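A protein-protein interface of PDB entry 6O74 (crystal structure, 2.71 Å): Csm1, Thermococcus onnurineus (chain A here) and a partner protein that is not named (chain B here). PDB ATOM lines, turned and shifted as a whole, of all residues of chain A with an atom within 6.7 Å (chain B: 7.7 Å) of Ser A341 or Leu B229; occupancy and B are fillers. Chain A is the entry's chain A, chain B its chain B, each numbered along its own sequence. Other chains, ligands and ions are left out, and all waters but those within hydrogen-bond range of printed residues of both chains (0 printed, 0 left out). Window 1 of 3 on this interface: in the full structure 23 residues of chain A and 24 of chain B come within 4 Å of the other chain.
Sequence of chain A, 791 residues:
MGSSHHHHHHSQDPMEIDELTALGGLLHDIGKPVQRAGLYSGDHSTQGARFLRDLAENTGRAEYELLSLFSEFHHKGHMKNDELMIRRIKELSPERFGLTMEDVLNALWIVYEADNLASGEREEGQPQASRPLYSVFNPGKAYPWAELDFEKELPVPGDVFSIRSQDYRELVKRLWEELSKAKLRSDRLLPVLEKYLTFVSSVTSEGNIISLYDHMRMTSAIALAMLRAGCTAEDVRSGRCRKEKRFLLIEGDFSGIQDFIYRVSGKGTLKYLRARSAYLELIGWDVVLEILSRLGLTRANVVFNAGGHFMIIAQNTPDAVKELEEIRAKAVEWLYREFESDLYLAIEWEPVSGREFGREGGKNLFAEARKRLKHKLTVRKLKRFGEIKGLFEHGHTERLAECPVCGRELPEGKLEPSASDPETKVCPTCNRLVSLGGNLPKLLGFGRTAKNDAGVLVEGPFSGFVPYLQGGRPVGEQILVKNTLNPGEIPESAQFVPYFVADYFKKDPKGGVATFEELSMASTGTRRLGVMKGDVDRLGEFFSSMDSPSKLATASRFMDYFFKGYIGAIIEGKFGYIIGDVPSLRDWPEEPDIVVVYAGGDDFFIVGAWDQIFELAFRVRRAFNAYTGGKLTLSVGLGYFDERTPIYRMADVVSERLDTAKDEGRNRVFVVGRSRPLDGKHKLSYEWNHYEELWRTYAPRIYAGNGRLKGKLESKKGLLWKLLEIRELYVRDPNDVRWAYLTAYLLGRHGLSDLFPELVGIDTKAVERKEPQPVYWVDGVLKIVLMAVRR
Ser A341 touches just one residue of chain B: Leu B229 (3.7 Å). Of the printed residues of chain A, Leu B229 touches Ser A341 (3.7 Å), Arg A384 (3.6 Å) and Phe A385 (3.6 Å). Of the printed residues of chain A, Pro B220 touches Phe A392 (3.2 Å). Of the printed residues of chain A, Pro B224 touches Phe A392 (3.4 Å). Of the printed residues of chain B, Phe A385 touches Leu B229. Of the printed residues of chain B, Phe A392 touches Pro B220 and Pro B224. Of the printed residues of chain B, Glu A340 touches Arg B231. Asp A342 touches none of the printed residues of chain B. Lys B232 touches none of the printed residues of chain A. The nearest residue of chain A that does not touch Leu B229 is Phe A392 (4.2 Å). The nearest printed residue of chain B that does not touch Phe A392 is Leu B229 (4.2 Å).
The backbone carbonyl oxygen of Arg A384 is in hydrogen-bond range of the indole nitrogen of Trp B227 (3.2 Å). The side-chain carboxylate (OE1) of Glu A340 is in salt-bridge range of the guanidinium group (NE) of Arg B231 (3.7 Å). OG1 of Thr B245 sits at hydrogen-bond distance from O of Leu A391, at 3.4 Å.
Of the 15 printed residues of chain A, 8 touch a printed residue of chain B. Hydrophobic or aromatic side chains of chain A that line the printed part of chain B: Tyr A336, Phe A385 and Phe A392. Printed residues of chain B that touch a printed residue of chain A: Pro B220, Pro B224, Trp B227, Leu B229, Arg B231 and Thr B245. Among the printed residues, 11 pairs touch across the chains.
OG of Ser A255 is in hydrogen-bond range of NH1 of Arg A384, at 3.2 Å. The backbone carbonyl oxygen of Ser A341 lies within hydrogen-bond range of the guanidinium group of Arg A384, at 2.6 Å. The backbone carbonyl oxygen (O) of Asp A342 sits at hydrogen-bond distance from the guanidinium group (NH2) of Arg A384.
Among the printed residues, merely in contact across the chains: Phe A392 with Pro B220 (3.2 Å), Phe A392 with Pro B224 (3.4 Å), Arg A384 with Leu B229 (3.6 Å), Tyr A336 with Arg B231 (3.6 Å), Phe A385 with Leu B229 (3.6 Å), Gly A386 with Trp B227 (3.7 Å), Tyr A336 with Thr B245 (3.7 Å) and Ser A341 with Leu B229 (3.7 Å).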
ATOM      1  N   SER A 255      -5.758 -26.444  22.402  1.00  0.00           N
ATOM      2  CA  SER A 255      -7.063 -27.106  22.652  1.00  0.00           C
ATOM      3  C   SER A 255      -7.293 -28.193  21.596  1.00  0.00           C
ATOM      4  O   SER A 255      -7.208 -27.883  20.392  1.00  0.00           O
ATOM      5  CB  SER A 255      -8.182 -26.099  22.674  1.00  0.00           C
ATOM      6  OG  SER A 255      -9.393 -26.703  23.100  1.00  0.00           O
ATOM      7  N   GLY A 256      -7.559 -29.422  22.043  1.00  0.00           N
ATOM      8  CA  GLY A 256      -7.784 -30.593  21.179  1.00  0.00           C
ATOM      9  C   GLY A 256      -6.517 -31.402  20.974  1.00  0.00           C
ATOM     10  O   GLY A 256      -6.441 -32.131  19.961  1.00  0.00           O
ATOM     11  N   LEU A 335      -3.177 -23.121  11.773  1.00  0.00           N
ATOM     12  CA  LEU A 335      -3.648 -24.372  12.425  1.00  0.00           C
ATOM     13  C   LEU A 335      -4.889 -24.872  11.681  1.00  0.00           C
ATOM     14  O   LEU A 335      -4.942 -26.085  11.391  1.00  0.00           O
ATOM     15  CB  LEU A 335      -3.955 -24.122  13.907  1.00  0.00           C
ATOM     16  CG  LEU A 335      -2.748 -24.058  14.841  1.00  0.00           C
ATOM     17  CD1 LEU A 335      -3.158 -23.562  16.223  1.00  0.00           C
ATOM     18  CD2 LEU A 335      -2.061 -25.415  14.947  1.00  0.00           C
ATOM     19  N   TYR A 336      -5.830 -23.971  11.368  1.00  0.00           N
ATOM     20  CA  TYR A 336      -7.092 -24.304  10.659  1.00  0.00           C
ATOM     21  C   TYR A 336      -6.760 -24.887   9.282  1.00  0.00           C
ATOM     22  O   TYR A 336      -7.244 -25.988   8.980  1.00  0.00           O
ATOM     23  CB  TYR A 336      -8.026 -23.098  10.547  1.00  0.00           C
ATOM     24  CG  TYR A 336      -9.415 -23.467  10.089  1.00  0.00           C
ATOM     25  CD1 TYR A 336      -9.766 -23.427   8.747  1.00  0.00           C
ATOM     26  CD2 TYR A 336     -10.370 -23.901  10.994  1.00  0.00           C
ATOM     27  CE1 TYR A 336     -11.035 -23.786   8.321  1.00  0.00           C
ATOM     28  CE2 TYR A 336     -11.643 -24.267  10.584  1.00  0.00           C
ATOM     29  CZ  TYR A 336     -11.978 -24.209   9.242  1.00  0.00           C
ATOM     30  OH  TYR A 336     -13.234 -24.564   8.839  1.00  0.00           O
ATOM     31  N   PHE A 339      -4.909 -28.592   9.890  1.00  0.00           N
ATOM     32  CA  PHE A 339      -5.569 -29.726  10.599  1.00  0.00           C
ATOM     33  C   PHE A 339      -7.085 -29.533  10.767  1.00  0.00           C
ATOM     34  O   PHE A 339      -7.700 -30.384  11.451  1.00  0.00           O
ATOM     35  CB  PHE A 339      -4.948 -29.910  11.984  1.00  0.00           C
ATOM     36  CG  PHE A 339      -3.442 -29.875  12.003  1.00  0.00           C
ATOM     37  CD1 PHE A 339      -2.699 -30.876  11.397  1.00  0.00           C
ATOM     38  CD2 PHE A 339      -2.769 -28.838  12.625  1.00  0.00           C
ATOM     39  CE1 PHE A 339      -1.314 -30.841  11.410  1.00  0.00           C
ATOM     40  CE2 PHE A 339      -1.385 -28.809  12.647  1.00  0.00           C
ATOM     41  CZ  PHE A 339      -0.663 -29.809  12.040  1.00  0.00           C
ATOM     42  N   GLU A 340      -7.671 -28.485  10.173  1.00  0.00           N
ATOM     43  CA  GLU A 340      -9.115 -28.130  10.303  1.00  0.00           C
ATOM     44  C   GLU A 340      -9.372 -27.679  11.747  1.00  0.00           C
ATOM     45  O   GLU A 340      -8.517 -26.970  12.304  1.00  0.00           O
ATOM     46  CB  GLU A 340      -9.998 -29.313   9.884  1.00  0.00           C
ATOM     47  CG  GLU A 340      -9.560 -29.995   8.597  1.00  0.00           C
ATOM     48  CD  GLU A 340      -9.661 -31.511   8.637  1.00  0.00           C
ATOM     49  OE1 GLU A 340     -10.767 -32.018   8.927  1.00  0.00           O
ATOM     50  OE2 GLU A 340      -8.632 -32.181   8.394  1.00  0.00           O
ATOM     51  N   SER A 341     -10.490 -28.101  12.342  1.00  0.00           N
ATOM     52  CA  SER A 341     -10.904 -27.761  13.728  1.00  0.00           C
ATOM     53  C   SER A 341     -10.228 -28.673  14.767  1.00  0.00           C
ATOM     54  O   SER A 341     -10.589 -28.545  15.947  1.00  0.00           O
ATOM     55  CB  SER A 341     -12.409 -27.830  13.844  1.00  0.00           C
ATOM     56  OG  SER A 341     -12.814 -27.985  15.197  1.00  0.00           O
ATOM     57  N   ASP A 342      -9.305 -29.560  14.372  1.00  0.00           N
ATOM     58  CA  ASP A 342      -8.716 -30.593  15.274  1.00  0.00           C
ATOM     59  C   ASP A 342      -7.913 -29.933  16.397  1.00  0.00           C
ATOM     60  O   ASP A 342      -8.182 -30.240  17.580  1.00  0.00           O
ATOM     61  CB  ASP A 342      -7.799 -31.574  14.536  1.00  0.00           C
ATOM     62  CG  ASP A 342      -8.487 -32.854  14.100  1.00  0.00           C
ATOM     63  OD1 ASP A 342      -9.625 -33.090  14.548  1.00  0.00           O
ATOM     64  OD2 ASP A 342      -7.874 -33.607  13.317  1.00  0.00           O
ATOM     65  N   LEU A 343      -6.949 -29.090  16.031  1.00  0.00           N
ATOM     66  CA  LEU A 343      -6.012 -28.442  16.979  1.00  0.00           C
ATOM     67  C   LEU A 343      -6.193 -26.925  16.919  1.00  0.00           C
ATOM     68  O   LEU A 343      -5.998 -26.343  15.833  1.00  0.00           O
ATOM     69  CB  LEU A 343      -4.577 -28.846  16.629  1.00  0.00           C
ATOM     70  CG  LEU A 343      -3.514 -28.387  17.624  1.00  0.00           C
ATOM     71  CD1 LEU A 343      -3.815 -28.903  19.025  1.00  0.00           C
ATOM     72  CD2 LEU A 343      -2.132 -28.830  17.175  1.00  0.00           C
ATOM     73  N   TYR A 344      -6.553 -26.333  18.054  1.00  0.00           N
ATOM     74  CA  TYR A 344      -6.760 -24.879  18.243  1.00  0.00           C
ATOM     75  C   TYR A 344      -5.719 -24.352  19.233  1.00  0.00           C
ATOM     76  O   TYR A 344      -5.263 -25.145  20.080  1.00  0.00           O
ATOM     77  CB  TYR A 344      -8.162 -24.614  18.790  1.00  0.00           C
ATOM     78  CG  TYR A 344      -8.418 -23.164  19.082  1.00  0.00           C
ATOM     79  CD1 TYR A 344      -8.236 -22.213  18.094  1.00  0.00           C
ATOM     80  CD2 TYR A 344      -8.818 -22.735  20.335  1.00  0.00           C
ATOM     81  CE1 TYR A 344      -8.453 -20.869  18.339  1.00  0.00           C
ATOM     82  CE2 TYR A 344      -9.038 -21.391  20.596  1.00  0.00           C
ATOM     83  CZ  TYR A 344      -8.854 -20.458  19.593  1.00  0.00           C
ATOM     84  OH  TYR A 344      -9.064 -19.134  19.817  1.00  0.00           O
ATOM     85  N   ARG A 384     -13.616 -21.236  19.722  1.00  0.00           N
ATOM     86  CA  ARG A 384     -12.551 -21.902  18.921  1.00  0.00           C
ATOM     87  C   ARG A 384     -12.638 -21.421  17.471  1.00  0.00           C
ATOM     88  O   ARG A 384     -13.694 -21.594  16.834  1.00  0.00           O
ATOM     89  CB  ARG A 384     -12.640 -23.430  19.024  1.00  0.00           C
ATOM     90  CG  ARG A 384     -12.102 -23.976  20.342  1.00  0.00           C
ATOM     91  CD  ARG A 384     -11.997 -25.487  20.475  1.00  0.00           C
ATOM     92  NE  ARG A 384     -11.306 -26.148  19.368  1.00  0.00           N
ATOM     93  CZ  ARG A 384     -10.734 -27.348  19.435  1.00  0.00           C
ATOM     94  NH1 ARG A 384     -10.747 -28.046  20.559  1.00  0.00           N
ATOM     95  NH2 ARG A 384     -10.134 -27.854  18.375  1.00  0.00           N
ATOM     96  N   PHE A 385     -11.558 -20.807  16.994  1.00  0.00           N
ATOM     97  CA  PHE A 385     -11.366 -20.319  15.606  1.00  0.00           C
ATOM     98  C   PHE A 385     -12.234 -19.080  15.344  1.00  0.00           C
ATOM     99  O   PHE A 385     -12.344 -18.686  14.170  1.00  0.00           O
ATOM    100  CB  PHE A 385     -11.616 -21.457  14.617  1.00  0.00           C
ATOM    101  CG  PHE A 385     -10.603 -22.565  14.708  1.00  0.00           C
ATOM    102  CD1 PHE A 385      -9.331 -22.399  14.185  1.00  0.00           C
ATOM    103  CD2 PHE A 385     -10.911 -23.766  15.318  1.00  0.00           C
ATOM    104  CE1 PHE A 385      -8.389 -23.413  14.267  1.00  0.00           C
ATOM    105  CE2 PHE A 385      -9.971 -24.784  15.393  1.00  0.00           C
ATOM    106  CZ  PHE A 385      -8.713 -24.606  14.866  1.00  0.00           C
ATOM    107  N   GLY A 386     -12.762 -18.452  16.405  1.00  0.00           N
ATOM    108  CA  GLY A 386     -13.479 -17.162  16.350  1.00  0.00           C
ATOM    109  C   GLY A 386     -12.670 -16.072  15.656  1.00  0.00           C
ATOM    110  O   GLY A 386     -13.292 -15.137  15.128  1.00  0.00           O
ATOM    111  N   LEU A 391     -15.132 -18.472   8.672  1.00  0.00           N
ATOM    112  CA  LEU A 391     -15.424 -19.780   9.315  1.00  0.00           C
ATOM    113  C   LEU A 391     -16.895 -20.158   9.097  1.00  0.00           C
ATOM    114  O   LEU A 391     -17.186 -21.370   9.068  1.00  0.00           O
ATOM    115  CB  LEU A 391     -15.095 -19.668  10.808  1.00  0.00           C
ATOM    116  CG  LEU A 391     -15.375 -20.911  11.652  1.00  0.00           C
ATOM    117  CD1 LEU A 391     -14.499 -22.079  11.216  1.00  0.00           C
ATOM    118  CD2 LEU A 391     -15.182 -20.607  13.131  1.00  0.00           C
ATOM    119  N   PHE A 392     -17.777 -19.161   8.954  1.00  0.00           N
ATOM    120  CA  PHE A 392     -19.255 -19.326   8.938  1.00  0.00           C
ATOM    121  C   PHE A 392     -19.834 -18.825   7.602  1.00  0.00           C
ATOM    122  O   PHE A 392     -20.533 -17.782   7.588  1.00  0.00           O
ATOM    123  CB  PHE A 392     -19.847 -18.620  10.162  1.00  0.00           C
ATOM    124  CG  PHE A 392     -19.361 -19.156  11.489  1.00  0.00           C
ATOM    125  CD1 PHE A 392     -19.426 -20.514  11.774  1.00  0.00           C
ATOM    126  CD2 PHE A 392     -18.846 -18.308  12.459  1.00  0.00           C
ATOM    127  CE1 PHE A 392     -18.993 -21.008  12.997  1.00  0.00           C
ATOM    128  CE2 PHE A 392     -18.403 -18.805  13.676  1.00  0.00           C
ATOM    129  CZ  PHE A 392     -18.479 -20.153  13.945  1.00  0.00           C
ATOM    130  N   LEU B  71     -23.816 -24.041  27.151  1.00  0.00           N
ATOM    131  CA  LEU B  71     -22.407 -23.580  27.274  1.00  0.00           C
ATOM    132  C   LEU B  71     -22.363 -22.242  28.018  1.00  0.00           C
ATOM    133  O   LEU B  71     -21.250 -21.764  28.281  1.00  0.00           O
ATOM    134  CB  LEU B  71     -21.783 -23.440  25.879  1.00  0.00           C
ATOM    135  CG  LEU B  71     -21.578 -24.740  25.099  1.00  0.00           C
ATOM    136  CD1 LEU B  71     -20.938 -24.473  23.745  1.00  0.00           C
ATOM    137  CD2 LEU B  71     -20.738 -25.730  25.882  1.00  0.00           C
ATOM    138  N   PRO B 220     -24.367 -21.288  11.421  1.00  0.00           N
ATOM    139  CA  PRO B 220     -24.682 -19.921  11.837  1.00  0.00           C
ATOM    140  C   PRO B 220     -24.515 -18.922  10.684  1.00  0.00           C
ATOM    141  O   PRO B 220     -23.742 -19.192   9.784  1.00  0.00           O
ATOM    142  CB  PRO B 220     -23.671 -19.675  12.961  1.00  0.00           C
ATOM    143  CG  PRO B 220     -22.489 -20.516  12.541  1.00  0.00           C
ATOM    144  CD  PRO B 220     -23.099 -21.782  11.982  1.00  0.00           C
ATOM    145  N   PRO B 224     -21.119 -16.559  16.593  1.00  0.00           N
ATOM    146  CA  PRO B 224     -21.918 -16.817  17.786  1.00  0.00           C
ATOM    147  C   PRO B 224     -21.217 -16.250  19.025  1.00  0.00           C
ATOM    148  O   PRO B 224     -20.146 -15.710  18.870  1.00  0.00           O
ATOM    149  CB  PRO B 224     -22.007 -18.349  17.841  1.00  0.00           C
ATOM    150  CG  PRO B 224     -20.903 -18.855  16.922  1.00  0.00           C
ATOM    151  CD  PRO B 224     -20.193 -17.659  16.319  1.00  0.00           C
ATOM    152  N   TRP B 227     -19.599 -21.377  21.773  1.00  0.00           N
ATOM    153  CA  TRP B 227     -19.915 -22.498  20.857  1.00  0.00           C
ATOM    154  C   TRP B 227     -18.868 -23.606  20.932  1.00  0.00           C
ATOM    155  O   TRP B 227     -17.741 -23.351  21.416  1.00  0.00           O
ATOM    156  CB  TRP B 227     -20.050 -21.970  19.429  1.00  0.00           C
ATOM    157  CG  TRP B 227     -18.753 -21.597  18.780  1.00  0.00           C
ATOM    158  CD1 TRP B 227     -17.929 -22.420  18.071  1.00  0.00           C
ATOM    159  CD2 TRP B 227     -18.152 -20.291  18.732  1.00  0.00           C
ATOM    160  NE1 TRP B 227     -16.851 -21.723  17.594  1.00  0.00           N
ATOM    161  CE2 TRP B 227     -16.961 -20.414  17.980  1.00  0.00           C
ATOM    162  CE3 TRP B 227     -18.501 -19.033  19.240  1.00  0.00           C
ATOM    163  CZ2 TRP B 227     -16.121 -19.327  17.731  1.00  0.00           C
ATOM    164  CZ3 TRP B 227     -17.670 -17.961  18.991  1.00  0.00           C
ATOM    165  CH2 TRP B 227     -16.496 -18.107  18.248  1.00  0.00           C
ATOM    166  N   ARG B 228     -19.271 -24.789  20.463  1.00  0.00           N
ATOM    167  CA  ARG B 228     -18.390 -25.925  20.109  1.00  0.00           C
ATOM    168  C   ARG B 228     -18.564 -26.196  18.613  1.00  0.00           C
ATOM    169  O   ARG B 228     -19.710 -26.384  18.171  1.00  0.00           O
ATOM    170  CB  ARG B 228     -18.734 -27.172  20.928  1.00  0.00           C
ATOM    171  CG  ARG B 228     -18.326 -27.095  22.390  1.00  0.00           C
ATOM    172  CD  ARG B 228     -18.068 -28.471  22.976  1.00  0.00           C
ATOM    173  NE  ARG B 228     -18.955 -29.494  22.427  1.00  0.00           N
ATOM    174  CZ  ARG B 228     -20.249 -29.639  22.725  1.00  0.00           C
ATOM    175  NH1 ARG B 228     -20.946 -30.611  22.158  1.00  0.00           N
ATOM    176  NH2 ARG B 228     -20.848 -28.818  23.577  1.00  0.00           N
ATOM    177  N   LEU B 229     -17.465 -26.207  17.864  1.00  0.00           N
ATOM    178  CA  LEU B 229     -17.462 -26.637  16.447  1.00  0.00           C
ATOM    179  C   LEU B 229     -17.760 -28.134  16.388  1.00  0.00           C
ATOM    180  O   LEU B 229     -17.413 -28.857  17.335  1.00  0.00           O
ATOM    181  CB  LEU B 229     -16.110 -26.314  15.807  1.00  0.00           C
ATOM    182  CG  LEU B 229     -15.791 -24.825  15.680  1.00  0.00           C
ATOM    183  CD1 LEU B 229     -14.427 -24.630  15.039  1.00  0.00           C
ATOM    184  CD2 LEU B 229     -16.870 -24.092  14.888  1.00  0.00           C
ATOM    185  N   LEU B 230     -18.379 -28.561  15.294  1.00  0.00           N
ATOM    186  CA  LEU B 230     -18.816 -29.956  15.059  1.00  0.00           C
ATOM    187  C   LEU B 230     -18.673 -30.225  13.558  1.00  0.00           C
ATOM    188  O   LEU B 230     -19.436 -29.626  12.775  1.00  0.00           O
ATOM    189  CB  LEU B 230     -20.253 -30.069  15.579  1.00  0.00           C
ATOM    190  CG  LEU B 230     -21.031 -31.326  15.204  1.00  0.00           C
ATOM    191  CD1 LEU B 230     -20.275 -32.589  15.601  1.00  0.00           C
ATOM    192  CD2 LEU B 230     -22.407 -31.292  15.852  1.00  0.00           C
ATOM    193  N   ARG B 231     -17.695 -31.055  13.183  1.00  0.00           N
ATOM    194  CA  ARG B 231     -17.197 -31.227  11.789  1.00  0.00           C
ATOM    195  C   ARG B 231     -17.934 -32.390  11.101  1.00  0.00           C
ATOM    196  O   ARG B 231     -17.954 -33.497  11.673  1.00  0.00           O
ATOM    197  CB  ARG B 231     -15.679 -31.447  11.842  1.00  0.00           C
ATOM    198  CG  ARG B 231     -14.985 -31.516  10.490  1.00  0.00           C
ATOM    199  CD  ARG B 231     -14.454 -30.179  10.011  1.00  0.00           C
ATOM    200  NE  ARG B 231     -14.022 -30.286   8.623  1.00  0.00           N
ATOM    201  CZ  ARG B 231     -13.848 -29.266   7.787  1.00  0.00           C
ATOM    202  NH1 ARG B 231     -14.062 -28.022   8.183  1.00  0.00           N
ATOM    203  NH2 ARG B 231     -13.460 -29.500   6.545  1.00  0.00           N
ATOM    204  N   LYS B 232     -18.517 -32.148   9.920  1.00  0.00           N
ATOM    205  CA  LYS B 232     -19.195 -33.181   9.087  1.00  0.00           C
ATOM    206  C   LYS B 232     -18.973 -32.874   7.603  1.00  0.00           C
ATOM    207  O   LYS B 232     -18.835 -33.849   6.840  1.00  0.00           O
ATOM    208  CB  LYS B 232     -20.691 -33.244   9.413  1.00  0.00           C
ATOM    209  CG  LYS B 232     -21.030 -33.944  10.723  1.00  0.00           C
ATOM    210  CD  LYS B 232     -22.515 -34.065  10.990  1.00  0.00           C
ATOM    211  CE  LYS B 232     -22.816 -34.665  12.348  1.00  0.00           C
ATOM    212  NZ  LYS B 232     -24.267 -34.887  12.545  1.00  0.00           N
ATOM    213  N   THR B 245     -19.247 -27.092   8.576  1.00  0.00           N
ATOM    214  CA  THR B 245     -18.903 -26.744   9.981  1.00  0.00           C
ATOM    215  C   THR B 245     -20.166 -26.298  10.727  1.00  0.00           C
ATOM    216  O   THR B 245     -20.648 -25.173  10.482  1.00  0.00           O
ATOM    217  CB  THR B 245     -17.796 -25.689  10.067  1.00  0.00           C
ATOM    218  OG1 THR B 245     -18.201 -24.557   9.298  1.00  0.00           O
ATOM    219  CG2 THR B 245     -16.460 -26.216   9.590  1.00  0.00           C
ATOM    220  N   PHE B 246     -20.655 -27.156  11.623  1.00  0.00           N
ATOM    221  CA  PHE B 246     -21.813 -26.897  12.514  1.00  0.00           C
ATOM    222  C   PHE B 246     -21.345 -26.369  13.875  1.00  0.00           C
ATOM    223  O   PHE B 246     -20.249 -26.707  14.359  1.00  0.00           O
ATOM    224  CB  PHE B 246     -22.643 -28.167  12.708  1.00  0.00           C
ATOM    225  CG  PHE B 246     -23.569 -28.496  11.567  1.00  0.00           C
ATOM    226  CD1 PHE B 246     -24.847 -27.961  11.518  1.00  0.00           C
ATOM    227  CD2 PHE B 246     -23.170 -29.350  10.551  1.00  0.00           C
ATOM    228  CE1 PHE B 246     -25.701 -28.269  10.472  1.00  0.00           C
ATOM    229  CE2 PHE B 246     -24.027 -29.657   9.507  1.00  0.00           C
ATOM    230  CZ  PHE B 246     -25.289 -29.113   9.468  1.00  0.00           C
ATOM    231  N   ILE B 247     -22.191 -25.516  14.447  1.00  0.00           N
ATOM    232  CA  ILE B 247     -22.259 -25.138  15.884  1.00  0.00           C
ATOM    233  C   ILE B 247     -22.998 -26.270  16.609  1.00  0.00           C
ATOM    234  O   ILE B 247     -24.063 -26.660  16.127  1.00  0.00           O
ATOM    235  CB  ILE B 247     -22.979 -23.777  15.979  1.00  0.00           C
ATOM    236  CG1 ILE B 247     -21.984 -22.624  15.980  1.00  0.00           C
ATOM    237  CG2 ILE B 247     -23.922 -23.672  17.163  1.00  0.00           C
ATOM    238  CD1 ILE B 247     -22.656 -21.312  15.729  1.00  0.00           C
ATOM    239  N   ALA B 248     -22.461 -26.778  17.718  1.00  0.00           N
ATOM    240  CA  ALA B 248     -23.050 -27.893  18.498  1.00  0.00           C
ATOM    241  C   ALA B 248     -24.309 -27.433  19.238  1.00  0.00           C
ATOM    242  O   ALA B 248     -24.457 -26.220  19.472  1.00  0.00           O
ATOM    243  CB  ALA B 248     -22.040 -28.430  19.479  1.00  0.00           C
ATOM    244  N   SER B 251     -24.665 -24.515  22.196  1.00  0.00           N
ATOM    245  CA  SER B 251     -24.003 -23.247  21.797  1.00  0.00           C
ATOM    246  C   SER B 251     -24.949 -22.073  22.069  1.00  0.00           C
ATOM    247  O   SER B 251     -26.158 -22.310  22.249  1.00  0.00           O
ATOM    248  CB  SER B 251     -23.578 -23.278  20.360  1.00  0.00           C
ATOM    249  OG  SER B 251     -22.853 -24.463  20.057  1.00  0.00           O
